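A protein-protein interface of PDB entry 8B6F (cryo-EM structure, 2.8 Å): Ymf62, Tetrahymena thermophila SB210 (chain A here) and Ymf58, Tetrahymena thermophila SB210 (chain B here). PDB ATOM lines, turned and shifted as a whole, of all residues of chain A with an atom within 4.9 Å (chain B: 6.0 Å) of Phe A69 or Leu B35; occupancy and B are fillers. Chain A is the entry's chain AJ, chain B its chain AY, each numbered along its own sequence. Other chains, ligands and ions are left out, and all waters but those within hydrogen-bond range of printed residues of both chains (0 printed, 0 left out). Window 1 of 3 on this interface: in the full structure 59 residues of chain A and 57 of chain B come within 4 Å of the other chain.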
ATOM      1  N   ILE A  42       5.153  -1.141   7.986  1.00  0.00           N
ATOM      2  CA  ILE A  42       5.906  -2.240   7.389  1.00  0.00           C
ATOM      3  C   ILE A  42       7.276  -1.746   6.943  1.00  0.00           C
ATOM      4  O   ILE A  42       8.308  -2.360   7.239  1.00  0.00           O
ATOM      5  CB  ILE A  42       5.116  -2.860   6.222  1.00  0.00           C
ATOM      6  CG1 ILE A  42       3.923  -3.653   6.760  1.00  0.00           C
ATOM      7  CG2 ILE A  42       6.018  -3.737   5.346  1.00  0.00           C
ATOM      8  CD1 ILE A  42       2.964  -4.126   5.693  1.00  0.00           C
ATOM      9  N   PHE A  46      11.132  -2.554   8.290  1.00  0.00           N
ATOM     10  CA  PHE A  46      12.256  -2.900   7.425  1.00  0.00           C
ATOM     11  C   PHE A  46      13.468  -2.032   7.736  1.00  0.00           C
ATOM     12  O   PHE A  46      14.595  -2.533   7.818  1.00  0.00           O
ATOM     13  CB  PHE A  46      11.866  -2.751   5.954  1.00  0.00           C
ATOM     14  CG  PHE A  46      10.883  -3.782   5.467  1.00  0.00           C
ATOM     15  CD1 PHE A  46      10.498  -4.847   6.267  1.00  0.00           C
ATOM     16  CD2 PHE A  46      10.356  -3.685   4.193  1.00  0.00           C
ATOM     17  CE1 PHE A  46       9.601  -5.787   5.804  1.00  0.00           C
ATOM     18  CE2 PHE A  46       9.460  -4.619   3.727  1.00  0.00           C
ATOM     19  CZ  PHE A  46       9.082  -5.672   4.532  1.00  0.00           C
ATOM     20  N   LEU A  49      15.015  -3.194  10.940  1.00  0.00           N
ATOM     21  CA  LEU A  49      15.798  -4.399  10.697  1.00  0.00           C
ATOM     22  C   LEU A  49      17.154  -4.056  10.095  1.00  0.00           C
ATOM     23  O   LEU A  49      18.171  -4.656  10.460  1.00  0.00           O
ATOM     24  CB  LEU A  49      15.029  -5.350   9.780  1.00  0.00           C
ATOM     25  CG  LEU A  49      13.833  -6.071  10.404  1.00  0.00           C
ATOM     26  CD1 LEU A  49      13.011  -6.769   9.334  1.00  0.00           C
ATOM     27  CD2 LEU A  49      14.292  -7.068  11.454  1.00  0.00           C
ATOM     28  N   ILE A  62      10.795  -8.839  13.561  1.00  0.00           N
ATOM     29  CA  ILE A  62      10.196  -9.859  12.705  1.00  0.00           C
ATOM     30  C   ILE A  62       8.803 -10.209  13.209  1.00  0.00           C
ATOM     31  O   ILE A  62       7.860 -10.357  12.425  1.00  0.00           O
ATOM     32  CB  ILE A  62      11.102 -11.104  12.634  1.00  0.00           C
ATOM     33  CG1 ILE A  62      12.431 -10.772  11.944  1.00  0.00           C
ATOM     34  CG2 ILE A  62      10.384 -12.256  11.927  1.00  0.00           C
ATOM     35  CD1 ILE A  62      12.346 -10.603  10.446  1.00  0.00           C
ATOM     36  N   GLU A  65       6.522  -7.472  12.293  1.00  0.00           N
ATOM     37  CA  GLU A  65       6.234  -7.564  10.867  1.00  0.00           C
ATOM     38  C   GLU A  65       5.168  -8.616  10.597  1.00  0.00           C
ATOM     39  O   GLU A  65       4.279  -8.413   9.763  1.00  0.00           O
ATOM     40  CB  GLU A  65       7.515  -7.889  10.098  1.00  0.00           C
ATOM     41  CG  GLU A  65       7.475  -7.487   8.641  1.00  0.00           C
ATOM     42  CD  GLU A  65       7.594  -5.992   8.454  1.00  0.00           C
ATOM     43  OE1 GLU A  65       8.672  -5.441   8.750  1.00  0.00           O
ATOM     44  OE2 GLU A  65       6.606  -5.367   8.022  1.00  0.00           O
ATOM     45  N   ILE A  66       5.239  -9.746  11.299  1.00  0.00           N
ATOM     46  CA  ILE A  66       4.200 -10.762  11.177  1.00  0.00           C
ATOM     47  C   ILE A  66       2.856 -10.199  11.615  1.00  0.00           C
ATOM     48  O   ILE A  66       1.823 -10.457  10.985  1.00  0.00           O
ATOM     49  CB  ILE A  66       4.584 -12.012  11.991  1.00  0.00           C
ATOM     50  CG1 ILE A  66       5.865 -12.629  11.430  1.00  0.00           C
ATOM     51  CG2 ILE A  66       3.457 -13.037  11.967  1.00  0.00           C
ATOM     52  CD1 ILE A  66       6.504 -13.649  12.342  1.00  0.00           C
ATOM     53  N   VAL A  67       2.841  -9.435  12.708  1.00  0.00           N
ATOM     54  CA  VAL A  67       1.594  -8.840  13.180  1.00  0.00           C
ATOM     55  C   VAL A  67       1.012  -7.909  12.123  1.00  0.00           C
ATOM     56  O   VAL A  67      -0.198  -7.915  11.869  1.00  0.00           O
ATOM     57  CB  VAL A  67       1.825  -8.109  14.516  1.00  0.00           C
ATOM     58  CG1 VAL A  67       0.598  -7.296  14.913  1.00  0.00           C
ATOM     59  CG2 VAL A  67       2.177  -9.103  15.611  1.00  0.00           C
ATOM     60  N   PHE A  68       1.860  -7.096  11.486  1.00  0.00           N
ATOM     61  CA  PHE A  68       1.365  -6.165  10.476  1.00  0.00           C
ATOM     62  C   PHE A  68       0.921  -6.886   9.211  1.00  0.00           C
ATOM     63  O   PHE A  68      -0.017  -6.439   8.542  1.00  0.00           O
ATOM     64  CB  PHE A  68       2.432  -5.119  10.155  1.00  0.00           C
ATOM     65  CG  PHE A  68       2.462  -3.978  11.127  1.00  0.00           C
ATOM     66  CD1 PHE A  68       1.529  -2.958  11.045  1.00  0.00           C
ATOM     67  CD2 PHE A  68       3.414  -3.928  12.128  1.00  0.00           C
ATOM     68  CE1 PHE A  68       1.549  -1.909  11.940  1.00  0.00           C
ATOM     69  CE2 PHE A  68       3.440  -2.882  13.028  1.00  0.00           C
ATOM     70  CZ  PHE A  68       2.507  -1.870  12.932  1.00  0.00           C
ATOM     71  N   PHE A  69       1.579  -7.990   8.856  1.00  0.00           N
ATOM     72  CA  PHE A  69       1.090  -8.806   7.749  1.00  0.00           C
ATOM     73  C   PHE A  69      -0.290  -9.362   8.063  1.00  0.00           C
ATOM     74  O   PHE A  69      -1.178  -9.367   7.203  1.00  0.00           O
ATOM     75  CB  PHE A  69       2.069  -9.941   7.453  1.00  0.00           C
ATOM     76  CG  PHE A  69       3.381  -9.487   6.868  1.00  0.00           C
ATOM     77  CD1 PHE A  69       3.631  -8.147   6.617  1.00  0.00           C
ATOM     78  CD2 PHE A  69       4.358 -10.413   6.549  1.00  0.00           C
ATOM     79  CE1 PHE A  69       4.833  -7.742   6.074  1.00  0.00           C
ATOM     80  CE2 PHE A  69       5.562 -10.012   6.006  1.00  0.00           C
ATOM     81  CZ  PHE A  69       5.798  -8.675   5.767  1.00  0.00           C
ATOM     82  N   GLY A  70      -0.486  -9.838   9.291  1.00  0.00           N
ATOM     83  CA  GLY A  70      -1.808 -10.277   9.703  1.00  0.00           C
ATOM     84  C   GLY A  70      -2.830  -9.158   9.655  1.00  0.00           C
ATOM     85  O   GLY A  70      -3.982  -9.372   9.273  1.00  0.00           O
ATOM     86  N   LEU A  71      -2.421  -7.949  10.039  1.00  0.00           N
ATOM     87  CA  LEU A  71      -3.319  -6.802   9.965  1.00  0.00           C
ATOM     88  C   LEU A  71      -3.732  -6.515   8.527  1.00  0.00           C
ATOM     89  O   LEU A  71      -4.904  -6.233   8.257  1.00  0.00           O
ATOM     90  CB  LEU A  71      -2.654  -5.571  10.585  1.00  0.00           C
ATOM     91  CG  LEU A  71      -2.519  -5.552  12.110  1.00  0.00           C
ATOM     92  CD1 LEU A  71      -1.745  -4.326  12.554  1.00  0.00           C
ATOM     93  CD2 LEU A  71      -3.877  -5.586  12.785  1.00  0.00           C
ATOM     94  N   PHE A  72      -2.786  -6.581   7.589  1.00  0.00           N
ATOM     95  CA  PHE A  72      -3.138  -6.394   6.185  1.00  0.00           C
ATOM     96  C   PHE A  72      -4.117  -7.460   5.720  1.00  0.00           C
ATOM     97  O   PHE A  72      -5.090  -7.158   5.019  1.00  0.00           O
ATOM     98  CB  PHE A  72      -1.891  -6.431   5.307  1.00  0.00           C
ATOM     99  CG  PHE A  72      -2.169  -6.889   3.905  1.00  0.00           C
ATOM    100  CD1 PHE A  72      -2.711  -6.023   2.974  1.00  0.00           C
ATOM    101  CD2 PHE A  72      -1.913  -8.197   3.528  1.00  0.00           C
ATOM    102  CE1 PHE A  72      -2.978  -6.445   1.688  1.00  0.00           C
ATOM    103  CE2 PHE A  72      -2.180  -8.627   2.243  1.00  0.00           C
ATOM    104  CZ  PHE A  72      -2.712  -7.748   1.321  1.00  0.00           C
ATOM    105  N   LEU A  73      -3.880  -8.714   6.100  1.00  0.00           N
ATOM    106  CA  LEU A  73      -4.788  -9.781   5.701  1.00  0.00           C
ATOM    107  C   LEU A  73      -6.176  -9.549   6.281  1.00  0.00           C
ATOM    108  O   LEU A  73      -7.186  -9.794   5.611  1.00  0.00           O
ATOM    109  CB  LEU A  73      -4.228 -11.131   6.147  1.00  0.00           C
ATOM    110  CG  LEU A  73      -3.016 -11.656   5.374  1.00  0.00           C
ATOM    111  CD1 LEU A  73      -2.479 -12.915   6.028  1.00  0.00           C
ATOM    112  CD2 LEU A  73      -3.353 -11.920   3.916  1.00  0.00           C
ATOM    113  N   LEU A  85      -1.712 -17.952   9.992  1.00  0.00           N
ATOM    114  CA  LEU A  85      -0.356 -17.415   9.969  1.00  0.00           C
ATOM    115  C   LEU A  85       0.141 -17.112  11.374  1.00  0.00           C
ATOM    116  O   LEU A  85       1.274 -17.452  11.731  1.00  0.00           O
ATOM    117  CB  LEU A  85      -0.320 -16.153   9.105  1.00  0.00           C
ATOM    118  CG  LEU A  85       0.965 -15.324   9.172  1.00  0.00           C
ATOM    119  CD1 LEU A  85       2.119 -16.090   8.597  1.00  0.00           C
ATOM    120  CD2 LEU A  85       0.792 -14.005   8.440  1.00  0.00           C
ATOM    121  N   TRP B   8       3.285  -5.167  -2.367  1.00  0.00           N
ATOM    122  CA  TRP B   8       3.807  -6.483  -2.013  1.00  0.00           C
ATOM    123  C   TRP B   8       4.883  -6.929  -2.992  1.00  0.00           C
ATOM    124  O   TRP B   8       5.893  -7.515  -2.586  1.00  0.00           O
ATOM    125  CB  TRP B   8       2.666  -7.496  -1.930  1.00  0.00           C
ATOM    126  CG  TRP B   8       1.853  -7.302  -0.689  1.00  0.00           C
ATOM    127  CD1 TRP B   8       0.641  -6.691  -0.591  1.00  0.00           C
ATOM    128  CD2 TRP B   8       2.211  -7.698   0.639  1.00  0.00           C
ATOM    129  NE1 TRP B   8       0.220  -6.687   0.717  1.00  0.00           N
ATOM    130  CE2 TRP B   8       1.166  -7.300   1.491  1.00  0.00           C
ATOM    131  CE3 TRP B   8       3.314  -8.354   1.187  1.00  0.00           C
ATOM    132  CZ2 TRP B   8       1.192  -7.537   2.863  1.00  0.00           C
ATOM    133  CZ3 TRP B   8       3.341  -8.588   2.549  1.00  0.00           C
ATOM    134  CH2 TRP B   8       2.284  -8.182   3.372  1.00  0.00           C
ATOM    135  N   ILE B  11       7.974  -5.043  -1.798  1.00  0.00           N
ATOM    136  CA  ILE B  11       8.514  -5.366  -0.482  1.00  0.00           C
ATOM    137  C   ILE B  11       9.118  -6.762  -0.439  1.00  0.00           C
ATOM    138  O   ILE B  11       9.998  -7.017   0.387  1.00  0.00           O
ATOM    139  CB  ILE B  11       7.454  -5.223   0.627  1.00  0.00           C
ATOM    140  CG1 ILE B  11       6.357  -6.272   0.461  1.00  0.00           C
ATOM    141  CG2 ILE B  11       6.919  -3.797   0.688  1.00  0.00           C
ATOM    142  CD1 ILE B  11       6.573  -7.489   1.340  1.00  0.00           C
ATOM    143  N   ILE B  15      12.703  -7.128   1.091  1.00  0.00           N
ATOM    144  CA  ILE B  15      13.066  -8.063   2.151  1.00  0.00           C
ATOM    145  C   ILE B  15      14.302  -8.859   1.756  1.00  0.00           C
ATOM    146  O   ILE B  15      15.204  -9.079   2.573  1.00  0.00           O
ATOM    147  CB  ILE B  15      11.874  -8.983   2.479  1.00  0.00           C
ATOM    148  CG1 ILE B  15      10.746  -8.174   3.124  1.00  0.00           C
ATOM    149  CG2 ILE B  15      12.296 -10.118   3.407  1.00  0.00           C
ATOM    150  CD1 ILE B  15       9.419  -8.895   3.160  1.00  0.00           C
ATOM    151  N   LEU B  30      18.505 -16.564   9.021  1.00  0.00           N
ATOM    152  CA  LEU B  30      17.376 -17.477   9.159  1.00  0.00           C
ATOM    153  C   LEU B  30      16.082 -16.715   9.415  1.00  0.00           C
ATOM    154  O   LEU B  30      15.040 -17.038   8.833  1.00  0.00           O
ATOM    155  CB  LEU B  30      17.651 -18.470  10.287  1.00  0.00           C
ATOM    156  CG  LEU B  30      16.701 -19.662  10.423  1.00  0.00           C
ATOM    157  CD1 LEU B  30      16.772 -20.562   9.200  1.00  0.00           C
ATOM    158  CD2 LEU B  30      17.017 -20.445  11.685  1.00  0.00           C
ATOM    159  N   PHE B  31      16.120 -15.713  10.292  1.00  0.00           N
ATOM    160  CA  PHE B  31      14.929 -14.902  10.531  1.00  0.00           C
ATOM    161  C   PHE B  31      14.491 -14.188   9.258  1.00  0.00           C
ATOM    162  O   PHE B  31      13.295 -14.122   8.953  1.00  0.00           O
ATOM    163  CB  PHE B  31      15.188 -13.889  11.648  1.00  0.00           C
ATOM    164  CG  PHE B  31      15.495 -14.513  12.984  1.00  0.00           C
ATOM    165  CD1 PHE B  31      15.256 -15.859  13.218  1.00  0.00           C
ATOM    166  CD2 PHE B  31      16.018 -13.744  14.009  1.00  0.00           C
ATOM    167  CE1 PHE B  31      15.537 -16.422  14.448  1.00  0.00           C
ATOM    168  CE2 PHE B  31      16.300 -14.302  15.239  1.00  0.00           C
ATOM    169  CZ  PHE B  31      16.060 -15.643  15.457  1.00  0.00           C
ATOM    170  N   MET B  32      15.447 -13.643   8.503  1.00  0.00           N
ATOM    171  CA  MET B  32      15.110 -12.947   7.266  1.00  0.00           C
ATOM    172  C   MET B  32      14.524 -13.903   6.234  1.00  0.00           C
ATOM    173  O   MET B  32      13.613 -13.534   5.487  1.00  0.00           O
ATOM    174  CB  MET B  32      16.346 -12.247   6.701  1.00  0.00           C
ATOM    175  CG  MET B  32      16.891 -11.134   7.587  1.00  0.00           C
ATOM    176  SD  MET B  32      15.691  -9.836   7.938  1.00  0.00           S
ATOM    177  CE  MET B  32      15.339  -9.242   6.289  1.00  0.00           C
ATOM    178  N   SER B  33      15.035 -15.134   6.174  1.00  0.00           N
ATOM    179  CA  SER B  33      14.457 -16.121   5.269  1.00  0.00           C
ATOM    180  C   SER B  33      13.021 -16.440   5.658  1.00  0.00           C
ATOM    181  O   SER B  33      12.151 -16.577   4.790  1.00  0.00           O
ATOM    182  CB  SER B  33      15.304 -17.393   5.265  1.00  0.00           C
ATOM    183  OG  SER B  33      15.319 -17.999   6.544  1.00  0.00           O
ATOM    184  N   GLU B  34      12.751 -16.566   6.958  1.00  0.00           N
ATOM    185  CA  GLU B  34      11.378 -16.780   7.402  1.00  0.00           C
ATOM    186  C   GLU B  34      10.487 -15.615   6.993  1.00  0.00           C
ATOM    187  O   GLU B  34       9.355 -15.819   6.540  1.00  0.00           O
ATOM    188  CB  GLU B  34      11.344 -16.974   8.919  1.00  0.00           C
ATOM    189  CG  GLU B  34       9.965 -17.291   9.474  1.00  0.00           C
ATOM    190  CD  GLU B  34       9.394 -18.578   8.916  1.00  0.00           C
ATOM    191  OE1 GLU B  34      10.174 -19.401   8.392  1.00  0.00           O
ATOM    192  OE2 GLU B  34       8.162 -18.767   8.995  1.00  0.00           O
ATOM    193  N   LEU B  35      10.979 -14.385   7.149  1.00  0.00           N
ATOM    194  CA  LEU B  35      10.201 -13.220   6.744  1.00  0.00           C
ATOM    195  C   LEU B  35       9.941 -13.227   5.242  1.00  0.00           C
ATOM    196  O   LEU B  35       8.852 -12.853   4.791  1.00  0.00           O
ATOM    197  CB  LEU B  35      10.920 -11.937   7.162  1.00  0.00           C
ATOM    198  CG  LEU B  35      10.256 -10.628   6.721  1.00  0.00           C
ATOM    199  CD1 LEU B  35       8.819 -10.553   7.212  1.00  0.00           C
ATOM    200  CD2 LEU B  35      11.051  -9.431   7.212  1.00  0.00           C
ATOM    201  N   THR B  36      10.930 -13.648   4.449  1.00  0.00           N
ATOM    202  CA  THR B  36      10.736 -13.739   3.006  1.00  0.00           C
ATOM    203  C   THR B  36       9.654 -14.752   2.657  1.00  0.00           C
ATOM    204  O   THR B  36       8.808 -14.494   1.794  1.00  0.00           O
ATOM    205  CB  THR B  36      12.049 -14.115   2.320  1.00  0.00           C
ATOM    206  OG1 THR B  36      13.076 -13.188   2.697  1.00  0.00           O
ATOM    207  CG2 THR B  36      11.889 -14.095   0.806  1.00  0.00           C
ATOM    208  N   TRP B  37       9.661 -15.910   3.316  1.00  0.00           N
ATOM    209  CA  TRP B  37       8.617 -16.897   3.071  1.00  0.00           C
ATOM    210  C   TRP B  37       7.244 -16.335   3.407  1.00  0.00           C
ATOM    211  O   TRP B  37       6.273 -16.571   2.681  1.00  0.00           O
ATOM    212  CB  TRP B  37       8.887 -18.165   3.881  1.00  0.00           C
ATOM    213  CG  TRP B  37       9.865 -19.087   3.235  1.00  0.00           C
ATOM    214  CD1 TRP B  37      11.089 -19.446   3.713  1.00  0.00           C
ATOM    215  CD2 TRP B  37       9.704 -19.771   1.986  1.00  0.00           C
ATOM    216  NE1 TRP B  37      11.700 -20.313   2.839  1.00  0.00           N
ATOM    217  CE2 TRP B  37      10.870 -20.528   1.772  1.00  0.00           C
ATOM    218  CE3 TRP B  37       8.684 -19.814   1.031  1.00  0.00           C
ATOM    219  CZ2 TRP B  37      11.046 -21.321   0.640  1.00  0.00           C
ATOM    220  CZ3 TRP B  37       8.858 -20.601  -0.092  1.00  0.00           C
ATOM    221  CH2 TRP B  37      10.032 -21.345  -0.279  1.00  0.00           C
ATOM    222  N   LEU B  38       7.144 -15.589   4.507  1.00  0.00           N
ATOM    223  CA  LEU B  38       5.862 -15.001   4.880  1.00  0.00           C
ATOM    224  C   LEU B  38       5.434 -13.911   3.907  1.00  0.00           C
ATOM    225  O   LEU B  38       4.234 -13.734   3.670  1.00  0.00           O
ATOM    226  CB  LEU B  38       5.931 -14.452   6.302  1.00  0.00           C
ATOM    227  CG  LEU B  38       6.187 -15.522   7.369  1.00  0.00           C
ATOM    228  CD1 LEU B  38       6.209 -14.916   8.761  1.00  0.00           C
ATOM    229  CD2 LEU B  38       5.202 -16.675   7.267  1.00  0.00           C
ATOM    230  N   ALA B  39       6.383 -13.164   3.345  1.00  0.00           N
ATOM    231  CA  ALA B  39       6.026 -12.200   2.311  1.00  0.00           C
ATOM    232  C   ALA B  39       5.445 -12.906   1.093  1.00  0.00           C
ATOM    233  O   ALA B  39       4.456 -12.445   0.512  1.00  0.00           O
ATOM    234  CB  ALA B  39       7.248 -11.369   1.921  1.00  0.00           C
ATOM    235  N   LEU B  40       6.051 -14.023   0.689  1.00  0.00           N
ATOM    236  CA  LEU B  40       5.489 -14.815  -0.399  1.00  0.00           C
ATOM    237  C   LEU B  40       4.102 -15.325  -0.039  1.00  0.00           C
ATOM    238  O   LEU B  40       3.196 -15.340  -0.879  1.00  0.00           O
ATOM    239  CB  LEU B  40       6.416 -15.987  -0.727  1.00  0.00           C
ATOM    240  CG  LEU B  40       7.525 -15.722  -1.747  1.00  0.00           C
ATOM    241  CD1 LEU B  40       8.470 -16.909  -1.822  1.00  0.00           C
ATOM    242  CD2 LEU B  40       6.947 -15.416  -3.117  1.00  0.00           C
ATOM    243  N   CYS B  42       1.875 -13.882   1.937  1.00  0.00           N
ATOM    244  CA  CYS B  42       0.927 -12.780   1.803  1.00  0.00           C
ATOM    245  C   CYS B  42       0.660 -12.445   0.339  1.00  0.00           C
ATOM    246  O   CYS B  42      -0.488 -12.208  -0.052  1.00  0.00           O
ATOM    247  CB  CYS B  42       1.450 -11.550   2.538  1.00  0.00           C
ATOM    248  SG  CYS B  42       1.737 -11.803   4.295  1.00  0.00           S
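Among the printed residues, pairs that only touch across the chains: Phe A72 with Trp B8, Phe A46 with Ile B15, Leu A85 with Leu B38, Phe A69 with Trp B8, Phe A69 with Leu B35, Ile A66 with Leu B38, Glu A65 with Leu B35, Ile A62 with Leu B35, Phe A69 with Cys B42, Phe A46 with Ile B11, Leu A49 with Leu B35 and Ile A62 with Phe B31.
Hydrophobic or aromatic side chains of chain B that line the printed part of chain A: Trp B8, Ile B11, Ile B15, Leu B35 and Leu B38.
Of the 14 printed residues of chain A, 8 touch a printed residue of chain B.
Hydrophobic or aromatic side chains of chain A that line the printed part of chain B: Phe A46, Leu A49, Ile A62, Ile A66, Phe A69, Phe A72 and Leu A85.
Among the printed residues, 12 pairs touch across the chains.
Among the printed residues, no Asp or Glu carboxylate lies within 4 Å of a Lys or Arg side-chain nitrogen of the other chain.
Of the printed residues of chain B, Glu A65 touches Leu B35 (3.6 Å).
Phe A69 touches three residues of chain B.
Of the printed residues of chain B, Leu A85 touches Leu B38.
Printed residues of chain A within 4 Å of Trp B8: Phe A69 and Phe A72.
Leu B35 touches four residues of chain A.
Of the printed residues of chain A, Leu B38 touches Ile A66 and Leu A85.
The nearest residue of chain A that does not touch Leu B35 is Phe A46 (4.2 Å).
The backbone carbonyl oxygen (O) of Leu B38 lies within hydrogen-bond range of the side-chain sulfur (SG) of Cys B42, at 3.2 Å.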
